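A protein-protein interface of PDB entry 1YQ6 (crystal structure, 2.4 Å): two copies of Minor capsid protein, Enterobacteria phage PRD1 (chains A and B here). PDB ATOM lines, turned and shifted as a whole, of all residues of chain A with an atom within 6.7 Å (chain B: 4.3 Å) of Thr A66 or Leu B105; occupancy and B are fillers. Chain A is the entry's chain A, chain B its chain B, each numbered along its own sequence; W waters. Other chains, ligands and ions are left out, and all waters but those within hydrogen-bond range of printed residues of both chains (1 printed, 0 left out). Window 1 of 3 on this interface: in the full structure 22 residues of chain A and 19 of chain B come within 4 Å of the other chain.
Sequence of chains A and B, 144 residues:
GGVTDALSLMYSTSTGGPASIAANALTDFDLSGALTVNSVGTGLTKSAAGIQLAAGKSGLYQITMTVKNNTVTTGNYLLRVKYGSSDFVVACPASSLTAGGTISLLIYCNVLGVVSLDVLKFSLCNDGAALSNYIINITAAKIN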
ATOM      1  N   GLN A  62     -26.018 -29.535   0.089  1.00  0.00           N
ATOM      2  CA  GLN A  62     -26.735 -28.898   1.184  1.00  0.00           C
ATOM      3  C   GLN A  62     -25.842 -27.743   1.617  1.00  0.00           C
ATOM      4  O   GLN A  62     -24.670 -27.939   1.940  1.00  0.00           O
ATOM      5  CB  GLN A  62     -26.947 -29.887   2.332  1.00  0.00           C
ATOM      6  CG  GLN A  62     -27.705 -29.318   3.532  1.00  0.00           C
ATOM      7  CD  GLN A  62     -29.037 -28.677   3.146  1.00  0.00           C
ATOM      8  OE1 GLN A  62     -29.883 -29.315   2.528  1.00  0.00           O
ATOM      9  NE2 GLN A  62     -29.223 -27.410   3.515  1.00  0.00           N
ATOM     10  N   ILE A  63     -26.396 -26.537   1.616  1.00  0.00           N
ATOM     11  CA  ILE A  63     -25.632 -25.351   1.952  1.00  0.00           C
ATOM     12  C   ILE A  63     -26.300 -24.463   2.991  1.00  0.00           C
ATOM     13  O   ILE A  63     -27.508 -24.271   2.971  1.00  0.00           O
ATOM     14  CB  ILE A  63     -25.400 -24.514   0.686  1.00  0.00           C
ATOM     15  CG1 ILE A  63     -24.763 -25.390  -0.392  1.00  0.00           C
ATOM     16  CG2 ILE A  63     -24.544 -23.309   0.997  1.00  0.00           C
ATOM     17  CD1 ILE A  63     -24.975 -24.892  -1.769  1.00  0.00           C
ATOM     18  N   THR A  64     -25.504 -23.916   3.900  1.00  0.00           N
ATOM     19  CA  THR A  64     -26.027 -23.020   4.909  1.00  0.00           C
ATOM     20  C   THR A  64     -25.044 -21.902   5.176  1.00  0.00           C
ATOM     21  O   THR A  64     -23.847 -22.123   5.271  1.00  0.00           O
ATOM     22  CB  THR A  64     -26.297 -23.734   6.254  1.00  0.00           C
ATOM     23  OG1 THR A  64     -27.479 -24.529   6.154  1.00  0.00           O
ATOM     24  CG2 THR A  64     -26.496 -22.720   7.364  1.00  0.00           C
ATOM     25  N   MET A  65     -25.560 -20.690   5.270  1.00  0.00           N
ATOM     26  CA  MET A  65     -24.734 -19.548   5.600  1.00  0.00           C
ATOM     27  C   MET A  65     -25.500 -18.769   6.643  1.00  0.00           C
ATOM     28  O   MET A  65     -26.676 -18.474   6.466  1.00  0.00           O
ATOM     29  CB  MET A  65     -24.471 -18.650   4.396  1.00  0.00           C
ATOM     30  CG  MET A  65     -23.733 -17.379   4.804  1.00  0.00           C
ATOM     31  SD  MET A  65     -23.102 -16.262   3.341  1.00  0.00           S
ATOM     32  CE  MET A  65     -24.799 -16.036   2.387  1.00  0.00           C
ATOM     33  N   THR A  66     -24.840 -18.458   7.746  1.00  0.00           N
ATOM     34  CA  THR A  66     -25.478 -17.702   8.807  1.00  0.00           C
ATOM     35  C   THR A  66     -24.605 -16.530   9.221  1.00  0.00           C
ATOM     36  O   THR A  66     -23.397 -16.535   9.000  1.00  0.00           O
ATOM     37  CB  THR A  66     -25.717 -18.573  10.036  1.00  0.00           C
ATOM     38  OG1 THR A  66     -24.501 -19.240  10.380  1.00  0.00           O
ATOM     39  CG2 THR A  66     -26.798 -19.596   9.764  1.00  0.00           C
ATOM     40  N   VAL A  67     -25.222 -15.523   9.820  1.00  0.00           N
ATOM     41  CA  VAL A  67     -24.481 -14.369  10.282  1.00  0.00           C
ATOM     42  C   VAL A  67     -25.059 -13.788  11.564  1.00  0.00           C
ATOM     43  O   VAL A  67     -26.270 -13.786  11.771  1.00  0.00           O
ATOM     44  CB  VAL A  67     -24.444 -13.234   9.207  1.00  0.00           C
ATOM     45  CG1 VAL A  67     -25.841 -12.743   8.899  1.00  0.00           C
ATOM     46  CG2 VAL A  67     -23.590 -12.084   9.699  1.00  0.00           C
ATOM     47  N   LYS A  68     -24.162 -13.318  12.426  1.00  0.00           N
ATOM     48  CA  LYS A  68     -24.529 -12.653  13.664  1.00  0.00           C
ATOM     49  C   LYS A  68     -23.606 -11.443  13.719  1.00  0.00           C
ATOM     50  O   LYS A  68     -22.401 -11.558  13.528  1.00  0.00           O
ATOM     51  CB  LYS A  68     -24.296 -13.535  14.908  1.00  0.00           C
ATOM     52  CG  LYS A  68     -25.308 -14.668  15.140  1.00  0.00           C
ATOM     53  CD  LYS A  68     -26.758 -14.186  15.152  1.00  0.00           C
ATOM     54  CE  LYS A  68     -27.022 -13.083  16.178  1.00  0.00           C
ATOM     55  NZ  LYS A  68     -26.825 -13.524  17.585  1.00  0.00           N
ATOM     56  N   LEU A  79     -28.995 -12.114   2.342  1.00  0.00           N
ATOM     57  CA  LEU A  79     -28.061 -13.203   2.081  1.00  0.00           C
ATOM     58  C   LEU A  79     -28.233 -13.761   0.682  1.00  0.00           C
ATOM     59  O   LEU A  79     -29.346 -13.857   0.177  1.00  0.00           O
ATOM     60  CB  LEU A  79     -28.233 -14.325   3.111  1.00  0.00           C
ATOM     61  CG  LEU A  79     -27.833 -13.990   4.547  1.00  0.00           C
ATOM     62  CD1 LEU A  79     -28.851 -13.053   5.157  1.00  0.00           C
ATOM     63  CD2 LEU A  79     -27.739 -15.262   5.358  1.00  0.00           C
ATOM     64  N   GLY A 100     -29.064 -10.816  12.849  1.00  0.00           N
ATOM     65  CA  GLY A 100     -28.391 -11.523  11.783  1.00  0.00           C
ATOM     66  C   GLY A 100     -29.392 -12.227  10.904  1.00  0.00           C
ATOM     67  O   GLY A 100     -30.542 -11.815  10.834  1.00  0.00           O
ATOM     68  N   GLY A 101     -28.966 -13.293  10.238  1.00  0.00           N
ATOM     69  CA  GLY A 101     -29.870 -14.004   9.356  1.00  0.00           C
ATOM     70  C   GLY A 101     -29.374 -15.379   8.968  1.00  0.00           C
ATOM     71  O   GLY A 101     -28.260 -15.776   9.323  1.00  0.00           O
ATOM     72  N   THR A 102     -30.198 -16.097   8.213  1.00  0.00           N
ATOM     73  CA  THR A 102     -29.868 -17.444   7.794  1.00  0.00           C
ATOM     74  C   THR A 102     -30.421 -17.801   6.420  1.00  0.00           C
ATOM     75  O   THR A 102     -31.516 -17.394   6.055  1.00  0.00           O
ATOM     76  CB  THR A 102     -30.450 -18.468   8.791  1.00  0.00           C
ATOM     77  OG1 THR A 102     -29.928 -18.221  10.099  1.00  0.00           O
ATOM     78  CG2 THR A 102     -30.120 -19.875   8.370  1.00  0.00           C
ATOM     79  N   ILE A 103     -29.648 -18.555   5.652  1.00  0.00           N
ATOM     80  CA  ILE A 103     -30.117 -19.038   4.367  1.00  0.00           C
ATOM     81  C   ILE A 103     -29.599 -20.461   4.221  1.00  0.00           C
ATOM     82  O   ILE A 103     -28.414 -20.716   4.417  1.00  0.00           O
ATOM     83  CB  ILE A 103     -29.643 -18.176   3.165  1.00  0.00           C
ATOM     84  CG1 ILE A 103     -30.336 -18.678   1.897  1.00  0.00           C
ATOM     85  CG2 ILE A 103     -28.128 -18.244   3.000  1.00  0.00           C
ATOM     86  CD1 ILE A 103     -30.154 -17.796   0.687  1.00  0.00           C
ATOM     87  N   SER A 104     -30.503 -21.389   3.932  1.00  0.00           N
ATOM     88  CA  SER A 104     -30.143 -22.790   3.756  1.00  0.00           C
ATOM     89  C   SER A 104     -30.716 -23.278   2.452  1.00  0.00           C
ATOM     90  O   SER A 104     -31.819 -22.897   2.080  1.00  0.00           O
ATOM     91  CB  SER A 104     -30.673 -23.640   4.899  1.00  0.00           C
ATOM     92  OG  SER A 104     -29.869 -23.447   6.034  1.00  0.00           O
ATOM     93  N   LEU A 124     -23.434 -11.445   1.813  1.00  0.00           N
ATOM     94  CA  LEU A 124     -24.503 -11.006   2.680  1.00  0.00           C
ATOM     95  C   LEU A 124     -24.185  -9.589   3.102  1.00  0.00           C
ATOM     96  O   LEU A 124     -23.089  -9.106   2.868  1.00  0.00           O
ATOM     97  CB  LEU A 124     -24.622 -11.923   3.904  1.00  0.00           C
ATOM     98  CG  LEU A 124     -23.485 -12.015   4.925  1.00  0.00           C
ATOM     99  CD1 LEU A 124     -23.438 -10.779   5.786  1.00  0.00           C
ATOM    100  CD2 LEU A 124     -23.717 -13.234   5.797  1.00  0.00           C
ATOM    101  N   ILE A 135     -19.811 -12.745  12.786  1.00  0.00           N
ATOM    102  CA  ILE A 135     -19.336 -14.119  12.859  1.00  0.00           C
ATOM    103  C   ILE A 135     -20.204 -14.752  11.788  1.00  0.00           C
ATOM    104  O   ILE A 135     -21.426 -14.739  11.883  1.00  0.00           O
ATOM    105  CB  ILE A 135     -19.622 -14.791  14.210  1.00  0.00           C
ATOM    106  CG1 ILE A 135     -18.755 -14.164  15.302  1.00  0.00           C
ATOM    107  CG2 ILE A 135     -19.341 -16.282  14.105  1.00  0.00           C
ATOM    108  CD1 ILE A 135     -17.255 -14.357  15.089  1.00  0.00           C
ATOM    109  N   ILE A 136     -19.569 -15.254  10.742  1.00  0.00           N
ATOM    110  CA  ILE A 136     -20.285 -15.865   9.637  1.00  0.00           C
ATOM    111  C   ILE A 136     -19.847 -17.307   9.522  1.00  0.00           C
ATOM    112  O   ILE A 136     -18.666 -17.615   9.639  1.00  0.00           O
ATOM    113  CB  ILE A 136     -19.980 -15.127   8.302  1.00  0.00           C
ATOM    114  CG1 ILE A 136     -20.624 -13.738   8.319  1.00  0.00           C
ATOM    115  CG2 ILE A 136     -20.472 -15.941   7.126  1.00  0.00           C
ATOM    116  CD1 ILE A 136     -20.311 -12.877   7.100  1.00  0.00           C
ATOM    117  N   ASN A 137     -20.806 -18.198   9.316  1.00  0.00           N
ATOM    118  CA  ASN A 137     -20.493 -19.606   9.164  1.00  0.00           C
ATOM    119  C   ASN A 137     -21.048 -20.066   7.831  1.00  0.00           C
ATOM    120  O   ASN A 137     -22.175 -19.749   7.484  1.00  0.00           O
ATOM    121  CB  ASN A 137     -21.092 -20.415  10.314  1.00  0.00           C
ATOM    122  CG  ASN A 137     -20.330 -20.225  11.618  1.00  0.00           C
ATOM    123  OD1 ASN A 137     -19.268 -20.818  11.828  1.00  0.00           O
ATOM    124  ND2 ASN A 137     -20.859 -19.385  12.490  1.00  0.00           N
ATOM    125  N   ILE A 138     -20.233 -20.787   7.074  1.00  0.00           N
ATOM    126  CA  ILE A 138     -20.642 -21.296   5.779  1.00  0.00           C
ATOM    127  C   ILE A 138     -20.288 -22.767   5.727  1.00  0.00           C
ATOM    128  O   ILE A 138     -19.130 -23.143   5.896  1.00  0.00           O
ATOM    129  CB  ILE A 138     -19.924 -20.557   4.632  1.00  0.00           C
ATOM    130  CG1 ILE A 138     -20.339 -19.083   4.620  1.00  0.00           C
ATOM    131  CG2 ILE A 138     -20.262 -21.202   3.311  1.00  0.00           C
ATOM    132  CD1 ILE A 138     -19.494 -18.221   3.715  1.00  0.00           C
ATOM    133  N   THR A 139     -21.296 -23.603   5.509  1.00  0.00           N
ATOM    134  CA  THR A 139     -21.082 -25.033   5.430  1.00  0.00           C
ATOM    135  C   THR A 139     -21.741 -25.590   4.184  1.00  0.00           C
ATOM    136  O   THR A 139     -22.875 -25.242   3.859  1.00  0.00           O
ATOM    137  CB  THR A 139     -21.681 -25.755   6.640  1.00  0.00           C
ATOM    138  OG1 THR A 139     -21.122 -25.224   7.843  1.00  0.00           O
ATOM    139  CG2 THR A 139     -21.389 -27.238   6.567  1.00  0.00           C
ATOM    140  N   TYR B  61     -24.685 -31.641  11.396  1.00  0.00           N
ATOM    141  CA  TYR B  61     -26.090 -31.809  11.736  1.00  0.00           C
ATOM    142  C   TYR B  61     -27.039 -30.933  10.926  1.00  0.00           C
ATOM    143  O   TYR B  61     -26.804 -29.740  10.753  1.00  0.00           O
ATOM    144  CB  TYR B  61     -26.311 -31.535  13.228  1.00  0.00           C
ATOM    145  CG  TYR B  61     -25.777 -32.618  14.131  1.00  0.00           C
ATOM    146  CD1 TYR B  61     -24.413 -32.735  14.375  1.00  0.00           C
ATOM    147  CD2 TYR B  61     -26.637 -33.555  14.711  1.00  0.00           C
ATOM    148  CE1 TYR B  61     -23.910 -33.760  15.172  1.00  0.00           C
ATOM    149  CE2 TYR B  61     -26.150 -34.585  15.511  1.00  0.00           C
ATOM    150  CZ  TYR B  61     -24.783 -34.681  15.733  1.00  0.00           C
ATOM    151  OH  TYR B  61     -24.276 -35.703  16.495  1.00  0.00           O
ATOM    152  N   GLN B  62     -28.111 -31.542  10.433  1.00  0.00           N
ATOM    153  CA  GLN B  62     -29.124 -30.828   9.668  1.00  0.00           C
ATOM    154  C   GLN B  62     -30.255 -30.587  10.662  1.00  0.00           C
ATOM    155  O   GLN B  62     -30.765 -31.520  11.279  1.00  0.00           O
ATOM    156  CB  GLN B  62     -29.598 -31.680   8.486  1.00  0.00           C
ATOM    157  CG  GLN B  62     -30.668 -31.019   7.614  1.00  0.00           C
ATOM    158  CD  GLN B  62     -30.252 -29.637   7.124  1.00  0.00           C
ATOM    159  OE1 GLN B  62     -29.208 -29.483   6.492  1.00  0.00           O
ATOM    160  NE2 GLN B  62     -31.072 -28.626   7.418  1.00  0.00           N
ATOM    161  N   ILE B  63     -30.639 -29.329  10.822  1.00  0.00           N
ATOM    162  CA  ILE B  63     -31.668 -28.970  11.779  1.00  0.00           C
ATOM    163  C   ILE B  63     -32.761 -28.089  11.195  1.00  0.00           C
ATOM    164  O   ILE B  63     -32.497 -27.205  10.394  1.00  0.00           O
ATOM    165  CB  ILE B  63     -31.027 -28.220  12.961  1.00  0.00           C
ATOM    166  CG1 ILE B  63     -29.895 -29.066  13.543  1.00  0.00           C
ATOM    167  CG2 ILE B  63     -32.069 -27.885  14.006  1.00  0.00           C
ATOM    168  CD1 ILE B  63     -28.892 -28.279  14.309  1.00  0.00           C
ATOM    169  N   VAL B  81     -31.619 -21.019  17.147  1.00  0.00           N
ATOM    170  CA  VAL B  81     -31.063 -22.323  17.455  1.00  0.00           C
ATOM    171  C   VAL B  81     -29.668 -22.054  17.997  1.00  0.00           C
ATOM    172  O   VAL B  81     -28.942 -21.223  17.458  1.00  0.00           O
ATOM    173  CB  VAL B  81     -30.958 -23.223  16.206  1.00  0.00           C
ATOM    174  CG1 VAL B  81     -30.256 -24.517  16.556  1.00  0.00           C
ATOM    175  CG2 VAL B  81     -32.339 -23.520  15.671  1.00  0.00           C
ATOM    176  N   PHE B  88     -27.800 -19.229  15.972  1.00  0.00           N
ATOM    177  CA  PHE B  88     -28.242 -18.885  14.628  1.00  0.00           C
ATOM    178  C   PHE B  88     -29.659 -18.356  14.706  1.00  0.00           C
ATOM    179  O   PHE B  88     -30.489 -18.907  15.424  1.00  0.00           O
ATOM    180  CB  PHE B  88     -28.161 -20.125  13.740  1.00  0.00           C
ATOM    181  CG  PHE B  88     -26.901 -20.913  13.938  1.00  0.00           C
ATOM    182  CD1 PHE B  88     -26.863 -21.971  14.831  1.00  0.00           C
ATOM    183  CD2 PHE B  88     -25.734 -20.559  13.276  1.00  0.00           C
ATOM    184  CE1 PHE B  88     -25.682 -22.666  15.067  1.00  0.00           C
ATOM    185  CE2 PHE B  88     -24.544 -21.255  13.510  1.00  0.00           C
ATOM    186  CZ  PHE B  88     -24.527 -22.309  14.409  1.00  0.00           C
ATOM    187  N   SER B 104     -33.768 -23.329   9.070  1.00  0.00           N
ATOM    188  CA  SER B 104     -33.094 -24.588   8.771  1.00  0.00           C
ATOM    189  C   SER B 104     -31.603 -24.345   8.761  1.00  0.00           C
ATOM    190  O   SER B 104     -31.156 -23.300   8.327  1.00  0.00           O
ATOM    191  CB  SER B 104     -33.534 -25.140   7.424  1.00  0.00           C
ATOM    192  OG  SER B 104     -34.824 -25.701   7.538  1.00  0.00           O
ATOM    193  N   LEU B 105     -30.840 -25.325   9.233  1.00  0.00           N
ATOM    194  CA  LEU B 105     -29.395 -25.180   9.334  1.00  0.00           C
ATOM    195  C   LEU B 105     -28.600 -26.454   9.151  1.00  0.00           C
ATOM    196  O   LEU B 105     -29.035 -27.526   9.535  1.00  0.00           O
ATOM    197  CB  LEU B 105     -29.030 -24.651  10.724  1.00  0.00           C
ATOM    198  CG  LEU B 105     -29.689 -23.412  11.304  1.00  0.00           C
ATOM    199  CD1 LEU B 105     -29.577 -23.469  12.799  1.00  0.00           C
ATOM    200  CD2 LEU B 105     -29.033 -22.155  10.747  1.00  0.00           C
ATOM    201  N   LEU B 106     -27.420 -26.316   8.565  1.00  0.00           N
ATOM    202  CA  LEU B 106     -26.488 -27.419   8.426  1.00  0.00           C
ATOM    203  C   LEU B 106     -25.288 -26.855   9.178  1.00  0.00           C
ATOM    204  O   LEU B 106     -24.615 -25.957   8.687  1.00  0.00           O
ATOM    205  CB  LEU B 106     -26.108 -27.690   6.967  1.00  0.00           C
ATOM    206  CG  LEU B 106     -25.014 -28.763   6.831  1.00  0.00           C
ATOM    207  CD1 LEU B 106     -25.490 -30.049   7.456  1.00  0.00           C
ATOM    208  CD2 LEU B 106     -24.645 -28.989   5.381  1.00  0.00           C
ATOM    209  N   ILE B 107     -25.046 -27.350  10.386  1.00  0.00           N
ATOM    210  CA  ILE B 107     -23.938 -26.853  11.182  1.00  0.00           C
ATOM    211  C   ILE B 107     -23.019 -27.955  11.653  1.00  0.00           C
ATOM    212  O   ILE B 107     -23.396 -29.128  11.666  1.00  0.00           O
ATOM    213  CB  ILE B 107     -24.439 -26.102  12.435  1.00  0.00           C
ATOM    214  CG1 ILE B 107     -25.247 -27.056  13.319  1.00  0.00           C
ATOM    215  CG2 ILE B 107     -25.276 -24.916  12.026  1.00  0.00           C
ATOM    216  CD1 ILE B 107     -25.728 -26.440  14.606  1.00  0.00           C
HETATM  217  O   HOH W   1     -22.972 -24.036   9.494  1.00  0.00           O
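N of Leu B106 lies within hydrogen-bond range of OG1 of Thr A64. O of Ser B104 lies within hydrogen-bond range of OG of Ser A104.
The side-chain hydroxyl of Ser A104 sits at hydrogen-bond distance from the side-chain hydroxyl of Thr A64. N of Thr A64 is in hydrogen-bond range of O of Thr A139, 2.9 Å away. The backbone NH of Thr A66 sits at hydrogen-bond distance from the backbone carbonyl oxygen of Asn A137, 3.0 Å away. NE2 of Gln B62 is in hydrogen-bond range of O of Leu B105, 3.1 Å away. N of Ile B63 sits at hydrogen-bond distance from O of Leu B105, 2.7 Å away. The backbone carbonyl oxygen (O) of Val B81 sits at hydrogen-bond distance from the backbone NH (N) of Phe B88, 2.7 Å away.
Among the printed residues, pairs that only touch across the chains: Gln A62 with Gln B62 (3.3 Å), Gln A62 with Leu B106 (3.6 Å), Thr A64 with Leu B105 (3.7 Å), Thr A66 with Phe B88 (3.4 Å), Thr A66 with Leu B105 (3.5 Å), Thr A102 with Ser B104 (3.6 Å), Thr A102 with Leu B105 (3.5 Å), Ser A104 with Leu B105 (3.8 Å) and Thr A139 with Leu B106 (3.6 Å).
Thr A66 touches just these residues of chain B: Phe B88 and Leu B105. Of the printed residues of chain B, Ser A104 touches Ser B104 (2.6 Å) and Leu B105 (3.8 Å). Ile A136 touches none of the printed residues of chain B. Of the printed residues of chain B, Thr A139 touches Leu B106 (3.6 Å). Ile B63 touches none of the printed residues of chain A. Of chain A, only Thr A64, Thr A66, Thr A102 and Ser A104 come within 4 Å of Leu B105. The nearest printed residue of chain B that does not touch Thr A66 is Ser B104 (5.9 Å). The nearest residue of chain A that does not touch Leu B105 is Gln A62 (5.8 Å). The nearest printed residue of chain B that does not touch Ser A104 is Leu B106 (4.5 Å).
Of the 9 printed residues of chain B, 5 touch a printed residue of chain A. Printed residues of chain B that touch a printed residue of chain A: Gln B62, Phe B88, Ser B104, Leu B105 and Leu B106. Hydrophobic or aromatic side chains of chain B within 4 Å of the printed part of chain A: Phe B88, Leu B105 and Leu B106. Of the 19 printed residues of chain A, 6 touch a printed residue of chain B. Printed residues of chain A that touch a printed residue of chain B: Gln A62, Thr A64, Thr A66, Thr A102, Ser A104 and Thr A139. Among the printed residues, 11 pairs touch across the chains. Among the printed residues, no Asp or Glu carboxylate lies within 4 Å of a Lys or Arg side-chain nitrogen of the other chain.
Gln A62 touches its own counterpart, Gln B62. Ser A104 touches its own counterpart, Ser B104. Positions printed for both chains: 62, 63 and 104. Of the 11 pairs that touch across the chains among the printed residues, 2 have their exchanged pair printed and touching as well.
Water W1 lies within hydrogen-bond range of the backbone carbonyl oxygen (O) of Leu B106 (2.7 Å) and the side-chain hydroxyl (OG1) of Thr A139 (2.7 Å).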
